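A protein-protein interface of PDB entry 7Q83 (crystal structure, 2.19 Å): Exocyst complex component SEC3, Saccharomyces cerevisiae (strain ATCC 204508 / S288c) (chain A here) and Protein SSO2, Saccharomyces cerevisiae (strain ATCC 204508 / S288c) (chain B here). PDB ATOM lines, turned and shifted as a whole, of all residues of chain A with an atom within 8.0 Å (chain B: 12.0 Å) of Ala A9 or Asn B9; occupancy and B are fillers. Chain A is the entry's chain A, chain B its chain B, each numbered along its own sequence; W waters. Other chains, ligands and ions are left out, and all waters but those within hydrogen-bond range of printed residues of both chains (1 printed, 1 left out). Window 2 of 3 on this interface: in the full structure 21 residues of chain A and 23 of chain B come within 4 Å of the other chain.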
ATOM      1  N   ASN A   6      22.814  -9.435 -10.441  1.00  0.00           N
ATOM      2  CA  ASN A   6      23.104  -9.326 -11.866  1.00  0.00           C
ATOM      3  C   ASN A   6      21.815  -9.193 -12.667  1.00  0.00           C
ATOM      4  O   ASN A   6      21.190 -10.194 -13.015  1.00  0.00           O
ATOM      5  CB  ASN A   6      23.903 -10.541 -12.342  1.00  0.00           C
ATOM      6  CG  ASN A   6      24.562 -10.317 -13.686  1.00  0.00           C
ATOM      7  OD1 ASN A   6      24.238  -9.370 -14.404  1.00  0.00           O
ATOM      8  ND2 ASN A   6      25.495 -11.195 -14.034  1.00  0.00           N
ATOM      9  N   PHE A   7      21.425  -7.949 -12.964  1.00  0.00           N
ATOM     10  CA  PHE A   7      20.162  -7.727 -13.661  1.00  0.00           C
ATOM     11  C   PHE A   7      20.183  -8.320 -15.063  1.00  0.00           C
ATOM     12  O   PHE A   7      19.194  -8.919 -15.503  1.00  0.00           O
ATOM     13  CB  PHE A   7      19.842  -6.235 -13.729  1.00  0.00           C
ATOM     14  CG  PHE A   7      18.705  -5.914 -14.652  1.00  0.00           C
ATOM     15  CD1 PHE A   7      17.403  -6.239 -14.304  1.00  0.00           C
ATOM     16  CD2 PHE A   7      18.936  -5.320 -15.883  1.00  0.00           C
ATOM     17  CE1 PHE A   7      16.351  -5.959 -15.155  1.00  0.00           C
ATOM     18  CE2 PHE A   7      17.888  -5.038 -16.741  1.00  0.00           C
ATOM     19  CZ  PHE A   7      16.593  -5.357 -16.376  1.00  0.00           C
ATOM     20  N   LEU A   8      21.296  -8.163 -15.784  1.00  0.00           N
ATOM     21  CA  LEU A   8      21.345  -8.645 -17.159  1.00  0.00           C
ATOM     22  C   LEU A   8      21.300 -10.165 -17.227  1.00  0.00           C
ATOM     23  O   LEU A   8      20.734 -10.722 -18.174  1.00  0.00           O
ATOM     24  CB  LEU A   8      22.594  -8.114 -17.862  1.00  0.00           C
ATOM     25  CG  LEU A   8      22.502  -6.644 -18.276  1.00  0.00           C
ATOM     26  CD1 LEU A   8      23.759  -6.204 -19.008  1.00  0.00           C
ATOM     27  CD2 LEU A   8      21.263  -6.401 -19.128  1.00  0.00           C
ATOM     28  N   ALA A   9      21.880 -10.853 -16.241  1.00  0.00           N
ATOM     29  CA  ALA A   9      21.799 -12.310 -16.222  1.00  0.00           C
ATOM     30  C   ALA A   9      20.387 -12.772 -15.889  1.00  0.00           C
ATOM     31  O   ALA A   9      19.837 -13.654 -16.558  1.00  0.00           O
ATOM     32  CB  ALA A   9      22.801 -12.882 -15.220  1.00  0.00           C
ATOM     33  N   GLU A  10      19.779 -12.176 -14.860  1.00  0.00           N
ATOM     34  CA  GLU A  10      18.450 -12.602 -14.438  1.00  0.00           C
ATOM     35  C   GLU A  10      17.392 -12.232 -15.473  1.00  0.00           C
ATOM     36  O   GLU A  10      16.438 -12.990 -15.688  1.00  0.00           O
ATOM     37  CB  GLU A  10      18.117 -11.998 -13.073  1.00  0.00           C
ATOM     38  CG  GLU A  10      16.710 -12.290 -12.584  1.00  0.00           C
ATOM     39  CD  GLU A  10      16.503 -13.741 -12.182  1.00  0.00           C
ATOM     40  OE1 GLU A  10      17.499 -14.490 -12.081  1.00  0.00           O
ATOM     41  OE2 GLU A  10      15.335 -14.134 -11.968  1.00  0.00           O
ATOM     42  N   GLN A  11      17.538 -11.072 -16.121  1.00  0.00           N
ATOM     43  CA  GLN A  11      16.648 -10.738 -17.228  1.00  0.00           C
ATOM     44  C   GLN A  11      16.799 -11.741 -18.364  1.00  0.00           C
ATOM     45  O   GLN A  11      15.812 -12.120 -19.006  1.00  0.00           O
ATOM     46  CB  GLN A  11      16.921  -9.318 -17.731  1.00  0.00           C
ATOM     47  CG  GLN A  11      16.120  -8.940 -18.977  1.00  0.00           C
ATOM     48  CD  GLN A  11      16.412  -7.532 -19.471  1.00  0.00           C
ATOM     49  OE1 GLN A  11      17.473  -7.264 -20.037  1.00  0.00           O
ATOM     50  NE2 GLN A  11      15.466  -6.626 -19.259  1.00  0.00           N
ATOM     51  N   TYR A  12      18.031 -12.189 -18.618  1.00  0.00           N
ATOM     52  CA  TYR A  12      18.257 -13.190 -19.654  1.00  0.00           C
ATOM     53  C   TYR A  12      17.586 -14.512 -19.306  1.00  0.00           C
ATOM     54  O   TYR A  12      17.015 -15.172 -20.183  1.00  0.00           O
ATOM     55  CB  TYR A  12      19.757 -13.395 -19.871  1.00  0.00           C
ATOM     56  CG  TYR A  12      20.086 -14.266 -21.063  1.00  0.00           C
ATOM     57  CD1 TYR A  12      20.192 -15.647 -20.934  1.00  0.00           C
ATOM     58  CD2 TYR A  12      20.282 -13.710 -22.317  1.00  0.00           C
ATOM     59  CE1 TYR A  12      20.489 -16.445 -22.021  1.00  0.00           C
ATOM     60  CE2 TYR A  12      20.581 -14.499 -23.410  1.00  0.00           C
ATOM     61  CZ  TYR A  12      20.683 -15.865 -23.257  1.00  0.00           C
ATOM     62  OH  TYR A  12      20.981 -16.652 -24.344  1.00  0.00           O
ATOM     63  N   GLU A  13      17.653 -14.920 -18.035  1.00  0.00           N
ATOM     64  CA  GLU A  13      17.027 -16.176 -17.632  1.00  0.00           C
ATOM     65  C   GLU A  13      15.515 -16.106 -17.782  1.00  0.00           C
ATOM     66  O   GLU A  13      14.886 -17.061 -18.254  1.00  0.00           O
ATOM     67  CB  GLU A  13      17.395 -16.517 -16.186  1.00  0.00           C
ATOM     68  CG  GLU A  13      18.882 -16.683 -15.934  1.00  0.00           C
ATOM     69  CD  GLU A  13      19.423 -17.999 -16.452  1.00  0.00           C
ATOM     70  OE1 GLU A  13      18.614 -18.883 -16.809  1.00  0.00           O
ATOM     71  OE2 GLU A  13      20.663 -18.148 -16.501  1.00  0.00           O
ATOM     72  N   ARG A  14      14.914 -14.986 -17.378  1.00  0.00           N
ATOM     73  CA  ARG A  14      13.465 -14.850 -17.472  1.00  0.00           C
ATOM     74  C   ARG A  14      13.017 -14.719 -18.922  1.00  0.00           C
ATOM     75  O   ARG A  14      12.002 -15.304 -19.320  1.00  0.00           O
ATOM     76  CB  ARG A  14      12.997 -13.649 -16.656  1.00  0.00           C
ATOM     77  CG  ARG A  14      12.916 -13.901 -15.166  1.00  0.00           C
ATOM     78  CD  ARG A  14      12.267 -12.722 -14.464  1.00  0.00           C
ATOM     79  NE  ARG A  14      12.996 -11.488 -14.726  1.00  0.00           N
ATOM     80  CZ  ARG A  14      13.670 -10.806 -13.811  1.00  0.00           C
ATOM     81  NH1 ARG A  14      13.709 -11.200 -12.546  1.00  0.00           N
ATOM     82  NH2 ARG A  14      14.316  -9.703 -14.172  1.00  0.00           N
ATOM     83  N   ASP A  15      13.758 -13.954 -19.725  1.00  0.00           N
ATOM     84  CA  ASP A  15      13.405 -13.810 -21.133  1.00  0.00           C
ATOM     85  C   ASP A  15      13.529 -15.139 -21.870  1.00  0.00           C
ATOM     86  O   ASP A  15      12.623 -15.533 -22.615  1.00  0.00           O
ATOM     87  CB  ASP A  15      14.280 -12.738 -21.787  1.00  0.00           C
ATOM     88  CG  ASP A  15      13.938 -11.337 -21.314  1.00  0.00           C
ATOM     89  OD1 ASP A  15      12.911 -11.185 -20.621  1.00  0.00           O
ATOM     90  OD2 ASP A  15      14.692 -10.392 -21.631  1.00  0.00           O
ATOM     91  N   ARG A  16      14.640 -15.852 -21.663  1.00  0.00           N
ATOM     92  CA  ARG A  16      14.853 -17.115 -22.368  1.00  0.00           C
ATOM     93  C   ARG A  16      13.757 -18.122 -22.042  1.00  0.00           C
ATOM     94  O   ARG A  16      13.241 -18.800 -22.938  1.00  0.00           O
ATOM     95  CB  ARG A  16      16.228 -17.689 -22.020  1.00  0.00           C
ATOM     96  CG  ARG A  16      16.314 -19.208 -22.139  1.00  0.00           C
ATOM     97  CD  ARG A  16      17.754 -19.696 -22.233  1.00  0.00           C
ATOM     98  NE  ARG A  16      18.451 -19.648 -20.953  1.00  0.00           N
ATOM     99  CZ  ARG A  16      19.738 -19.924 -20.793  1.00  0.00           C
ATOM    100  NH1 ARG A  16      20.503 -20.270 -21.814  1.00  0.00           N
ATOM    101  NH2 ARG A  16      20.272 -19.852 -19.575  1.00  0.00           N
ATOM    102  N   THR A  40      19.819 -18.308 -28.651  1.00  0.00           N
ATOM    103  CA  THR A  40      20.059 -17.134 -27.817  1.00  0.00           C
ATOM    104  C   THR A  40      19.148 -16.005 -28.284  1.00  0.00           C
ATOM    105  O   THR A  40      18.346 -16.170 -29.206  1.00  0.00           O
ATOM    106  CB  THR A  40      21.532 -16.712 -27.848  1.00  0.00           C
ATOM    107  OG1 THR A  40      21.753 -15.691 -26.865  1.00  0.00           O
ATOM    108  CG2 THR A  40      21.914 -16.181 -29.220  1.00  0.00           C
ATOM    109  N   HIS A  41      19.283 -14.848 -27.636  1.00  0.00           N
ATOM    110  CA  HIS A  41      18.447 -13.695 -27.946  1.00  0.00           C
ATOM    111  C   HIS A  41      19.133 -12.432 -27.442  1.00  0.00           C
ATOM    112  O   HIS A  41      20.157 -12.487 -26.757  1.00  0.00           O
ATOM    113  CB  HIS A  41      17.054 -13.834 -27.325  1.00  0.00           C
ATOM    114  CG  HIS A  41      17.047 -13.669 -25.838  1.00  0.00           C
ATOM    115  ND1 HIS A  41      17.261 -14.720 -24.972  1.00  0.00           N
ATOM    116  CD2 HIS A  41      16.877 -12.571 -25.062  1.00  0.00           C
ATOM    117  CE1 HIS A  41      17.216 -14.279 -23.728  1.00  0.00           C
ATOM    118  NE2 HIS A  41      16.985 -12.978 -23.755  1.00  0.00           N
ATOM    119  N   VAL A 138      28.077  -8.827 -26.632  1.00  0.00           N
ATOM    120  CA  VAL A 138      27.720 -10.212 -26.343  1.00  0.00           C
ATOM    121  C   VAL A 138      26.905 -10.814 -27.482  1.00  0.00           C
ATOM    122  O   VAL A 138      27.158 -11.948 -27.908  1.00  0.00           O
ATOM    123  CB  VAL A 138      26.973 -10.296 -25.000  1.00  0.00           C
ATOM    124  CG1 VAL A 138      26.338 -11.668 -24.824  1.00  0.00           C
ATOM    125  CG2 VAL A 138      27.924  -9.990 -23.847  1.00  0.00           C
ATOM    126  N   ALA B   8      23.492 -21.768 -20.032  1.00  0.00           N
ATOM    127  CA  ALA B   8      24.167 -20.999 -21.068  1.00  0.00           C
ATOM    128  C   ALA B   8      23.752 -19.530 -21.025  1.00  0.00           C
ATOM    129  O   ALA B   8      23.166 -19.015 -21.978  1.00  0.00           O
ATOM    130  CB  ALA B   8      23.879 -21.590 -22.439  1.00  0.00           C
ATOM    131  N   ASN B   9      24.058 -18.858 -19.913  1.00  0.00           N
ATOM    132  CA  ASN B   9      23.762 -17.441 -19.759  1.00  0.00           C
ATOM    133  C   ASN B   9      25.006 -16.637 -20.112  1.00  0.00           C
ATOM    134  O   ASN B   9      25.947 -16.574 -19.305  1.00  0.00           O
ATOM    135  CB  ASN B   9      23.304 -17.133 -18.331  1.00  0.00           C
ATOM    136  CG  ASN B   9      22.689 -15.749 -18.195  1.00  0.00           C
ATOM    137  OD1 ASN B   9      23.115 -14.793 -18.845  1.00  0.00           O
ATOM    138  ND2 ASN B   9      21.681 -15.639 -17.339  1.00  0.00           N
ATOM    139  N   PRO B  10      25.066 -16.003 -21.287  1.00  0.00           N
ATOM    140  CA  PRO B  10      26.271 -15.253 -21.669  1.00  0.00           C
ATOM    141  C   PRO B  10      26.499 -13.991 -20.855  1.00  0.00           C
ATOM    142  O   PRO B  10      27.510 -13.313 -21.073  1.00  0.00           O
ATOM    143  CB  PRO B  10      26.014 -14.916 -23.145  1.00  0.00           C
ATOM    144  CG  PRO B  10      24.527 -14.875 -23.259  1.00  0.00           C
ATOM    145  CD  PRO B  10      24.013 -15.927 -22.314  1.00  0.00           C
ATOM    146  N   TYR B  11      25.603 -13.655 -19.932  1.00  0.00           N
ATOM    147  CA  TYR B  11      25.730 -12.476 -19.084  1.00  0.00           C
ATOM    148  C   TYR B  11      26.054 -12.866 -17.644  1.00  0.00           C
ATOM    149  O   TYR B  11      25.484 -12.322 -16.697  1.00  0.00           O
ATOM    150  CB  TYR B  11      24.456 -11.638 -19.140  1.00  0.00           C
ATOM    151  CG  TYR B  11      24.176 -11.061 -20.508  1.00  0.00           C
ATOM    152  CD1 TYR B  11      24.731  -9.848 -20.896  1.00  0.00           C
ATOM    153  CD2 TYR B  11      23.364 -11.731 -21.415  1.00  0.00           C
ATOM    154  CE1 TYR B  11      24.481  -9.316 -22.149  1.00  0.00           C
ATOM    155  CE2 TYR B  11      23.109 -11.204 -22.674  1.00  0.00           C
ATOM    156  CZ  TYR B  11      23.672  -9.996 -23.034  1.00  0.00           C
ATOM    157  OH  TYR B  11      23.425  -9.465 -24.282  1.00  0.00           O
ATOM    158  N   GLU B  12      26.980 -13.811 -17.477  1.00  0.00           N
ATOM    159  CA  GLU B  12      27.341 -14.372 -16.172  1.00  0.00           C
ATOM    160  C   GLU B  12      26.149 -15.093 -15.551  1.00  0.00           C
ATOM    161  O   GLU B  12      25.205 -15.460 -16.248  1.00  0.00           O
ATOM    162  CB  GLU B  12      27.857 -13.290 -15.217  1.00  0.00           C
ATOM    163  CG  GLU B  12      29.344 -12.998 -15.330  1.00  0.00           C
ATOM    164  CD  GLU B  12      30.173 -14.252 -15.527  1.00  0.00           C
ATOM    165  OE1 GLU B  12      30.319 -15.027 -14.558  1.00  0.00           O
ATOM    166  OE2 GLU B  12      30.683 -14.457 -16.649  1.00  0.00           O
ATOM    167  N   ARG B 127      43.245 -19.818 -23.072  1.00  0.00           N
ATOM    168  CA  ARG B 127      42.014 -20.271 -23.712  1.00  0.00           C
ATOM    169  C   ARG B 127      41.728 -19.479 -24.982  1.00  0.00           C
ATOM    170  O   ARG B 127      41.308 -20.050 -25.995  1.00  0.00           O
ATOM    171  CB  ARG B 127      40.847 -20.160 -22.733  1.00  0.00           C
ATOM    172  CG  ARG B 127      39.708 -21.127 -23.003  1.00  0.00           C
ATOM    173  CD  ARG B 127      38.519 -20.835 -22.104  1.00  0.00           C
ATOM    174  NE  ARG B 127      38.101 -19.442 -22.207  1.00  0.00           N
ATOM    175  CZ  ARG B 127      37.100 -19.013 -22.963  1.00  0.00           C
ATOM    176  NH1 ARG B 127      36.375 -19.847 -23.689  1.00  0.00           N
ATOM    177  NH2 ARG B 127      36.820 -17.713 -22.991  1.00  0.00           N
ATOM    178  N   ASN B 223      33.009 -25.791 -28.856  1.00  0.00           N
ATOM    179  CA  ASN B 223      31.954 -25.647 -27.861  1.00  0.00           C
ATOM    180  C   ASN B 223      32.412 -26.112 -26.485  1.00  0.00           C
ATOM    181  O   ASN B 223      32.029 -25.519 -25.472  1.00  0.00           O
ATOM    182  CB  ASN B 223      30.716 -26.421 -28.303  1.00  0.00           C
ATOM    183  CG  ASN B 223      29.923 -25.684 -29.361  1.00  0.00           C
ATOM    184  OD1 ASN B 223      30.081 -24.476 -29.543  1.00  0.00           O
ATOM    185  ND2 ASN B 223      29.065 -26.409 -30.070  1.00  0.00           N
ATOM    186  N   GLU B 226      34.171 -23.342 -24.720  1.00  0.00           N
ATOM    187  CA  GLU B 226      33.326 -22.251 -24.261  1.00  0.00           C
ATOM    188  C   GLU B 226      32.511 -22.616 -23.030  1.00  0.00           C
ATOM    189  O   GLU B 226      32.012 -21.715 -22.347  1.00  0.00           O
ATOM    190  CB  GLU B 226      32.387 -21.798 -25.384  1.00  0.00           C
ATOM    191  CG  GLU B 226      33.100 -21.375 -26.666  1.00  0.00           C
ATOM    192  CD  GLU B 226      33.583 -19.935 -26.633  1.00  0.00           C
ATOM    193  OE1 GLU B 226      33.955 -19.446 -25.544  1.00  0.00           O
ATOM    194  OE2 GLU B 226      33.588 -19.289 -27.702  1.00  0.00           O
ATOM    195  N   GLU B 227      32.362 -23.905 -22.736  1.00  0.00           N
ATOM    196  CA  GLU B 227      31.696 -24.314 -21.507  1.00  0.00           C
ATOM    197  C   GLU B 227      32.480 -23.819 -20.299  1.00  0.00           C
ATOM    198  O   GLU B 227      33.712 -23.878 -20.272  1.00  0.00           O
ATOM    199  CB  GLU B 227      31.556 -25.837 -21.453  1.00  0.00           C
ATOM    200  CG  GLU B 227      30.454 -26.409 -22.337  1.00  0.00           C
ATOM    201  CD  GLU B 227      30.498 -27.924 -22.405  1.00  0.00           C
ATOM    202  OE1 GLU B 227      31.122 -28.541 -21.514  1.00  0.00           O
ATOM    203  OE2 GLU B 227      29.914 -28.498 -23.348  1.00  0.00           O
ATOM    204  N   LEU B 228      31.757 -23.317 -19.301  1.00  0.00           N
ATOM    205  CA  LEU B 228      32.393 -22.843 -18.083  1.00  0.00           C
ATOM    206  C   LEU B 228      32.955 -24.015 -17.284  1.00  0.00           C
ATOM    207  O   LEU B 228      32.493 -25.152 -17.397  1.00  0.00           O
ATOM    208  CB  LEU B 228      31.399 -22.054 -17.224  1.00  0.00           C
ATOM    209  CG  LEU B 228      30.897 -20.697 -17.733  1.00  0.00           C
ATOM    210  CD1 LEU B 228      32.035 -19.882 -18.331  1.00  0.00           C
ATOM    211  CD2 LEU B 228      29.752 -20.854 -18.732  1.00  0.00           C
ATOM    212  N   VAL B 229      33.966 -23.725 -16.472  1.00  0.00           N
ATOM    213  CA  VAL B 229      34.603 -24.718 -15.615  1.00  0.00           C
ATOM    214  C   VAL B 229      34.220 -24.407 -14.175  1.00  0.00           C
ATOM    215  O   VAL B 229      34.455 -23.294 -13.689  1.00  0.00           O
ATOM    216  CB  VAL B 229      36.129 -24.734 -15.795  1.00  0.00           C
ATOM    217  CG1 VAL B 229      36.705 -26.043 -15.284  1.00  0.00           C
ATOM    218  CG2 VAL B 229      36.495 -24.524 -17.257  1.00  0.00           C
ATOM    219  N   ILE B 230      33.625 -25.384 -13.498  1.00  0.00           N
ATOM    220  CA  ILE B 230      33.226 -25.216 -12.105  1.00  0.00           C
ATOM    221  C   ILE B 230      33.601 -26.453 -11.297  1.00  0.00           C
ATOM    222  O   ILE B 230      34.734 -26.929 -11.367  1.00  0.00           O
ATOM    223  CB  ILE B 230      31.719 -24.922 -11.981  1.00  0.00           C
ATOM    224  CG1 ILE B 230      30.909 -25.893 -12.843  1.00  0.00           C
ATOM    225  CG2 ILE B 230      31.423 -23.479 -12.364  1.00  0.00           C
ATOM    226  CD1 ILE B 230      29.477 -26.081 -12.376  1.00  0.00           C
HETATM  227  O   HOH W   1      22.766 -11.554 -25.948  1.00  0.00           O
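The side-chain amide nitrogen (ND2) of Asn A6 lies within hydrogen-bond range of the backbone carbonyl oxygen (O) of Tyr B11 (2.9 Å).
The backbone carbonyl oxygen (O) of Ala A9 is in hydrogen-bond range of the side-chain amide nitrogen (ND2) of Asn B9 (2.8 Å).
OE2 of Glu A13 lies within hydrogen-bond range of ND2 of Asn B9, at 2.8 Å.
The guanidinium group (NH1) of Arg A16 sits at hydrogen-bond distance from the backbone carbonyl oxygen (O) of Ala B8 (2.9 Å).
The backbone NH (N) of Leu A8 lies close to the side-chain amide oxygen (OD1) of Asn A6, at 3.5 Å.
The side-chain amide oxygen of Asn A6 lies within hydrogen-bond range of the backbone NH of Ala A9.
OH of Tyr A12 sits at hydrogen-bond distance from OG1 of Thr A40.
OE1 of Glu A13 lies within salt-bridge range of NH2 of Arg A16 (3.4 Å).
The side-chain amide oxygen of Asn B9 sits at hydrogen-bond distance from the backbone NH of Tyr B11 (2.9 Å).
The side-chain amide oxygen (OD1) of Asn B9 sits close to the backbone carbonyl oxygen (O) of Glu B12 (3.4 Å).
Glu B12 touches Asn A6.
Tyr B11 touches Leu A8 (CB to O, 3.95 Å).
Ala A9 touches Tyr B11 (CB to O, 3.1 Å).
Ala A9 touches Glu B12.
O of Ala B8 touches CE1 of Tyr A12, 3.7 Å away.
Tyr A12 touches Asn B9 (CD1 to OD1, 3.7 Å).
Tyr A12 touches Tyr B11.
Asn B9 touches Arg A16.
Val A138 touches Pro B10 (CG1 to CB, 3.7 Å).
Tyr B11 touches Val A138.
Of chain A, only Ala A9 (2.8 Å), Tyr A12 (3.7 Å), Glu A13 (2.8 Å) and Arg A16 (3.9 Å) come within 4 Å of Asn B9.
Of chain B, only Tyr B11 and Glu B12 come within 4 Å of Asn A6.
Phe A7 touches none of the printed residues of chain B.
Glu A10 touches none of the printed residues of chain B.
Tyr A12 touches just these residues of chain B: Ala B8 (3.7 Å), Asn B9 (3.7 Å), Pro B10 (3.5 Å) and Tyr B11 (3.8 Å).
Glu A13 touches just one residue of chain B: Asn B9.
Ala B8 touches just these residues of chain A: Tyr A12 and Arg A16.
Of the printed residues of chain A, Glu B12 touches Asn A6 (3.4 Å) and Ala A9 (3.7 Å).
Of the printed residues of chain B, Val A138 touches Pro B10 (3.7 Å) and Tyr B11 (3.6 Å).
Of the printed residues of chain B, Arg A16 touches Ala B8 and Asn B9.
Ile B230 touches none of the printed residues of chain A.
Val B229 touches none of the printed residues of chain A.
Of the 12 printed residues of chain B, 5 touch a printed residue of chain A.
Along chain B the printed residues that touch a printed residue of chain A span positions 8 to 12.
Of the 14 printed residues of chain A, 7 touch a printed residue of chain B.
Printed residues of chain A that touch a printed residue of chain B: Asn A6, Leu A8, Ala A9, Tyr A12, Glu A13, Arg A16 and Val A138.
Along chain A the printed residues that touch a printed residue of chain B span positions 6 to 138.
Among the printed residues, no Asp or Glu carboxylate lies within 4 Å of a Lys or Arg side-chain nitrogen of the other chain.
Water W1 bridges OH of Tyr B11 (2.8 Å) and O of His A41 (2.9 Å).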
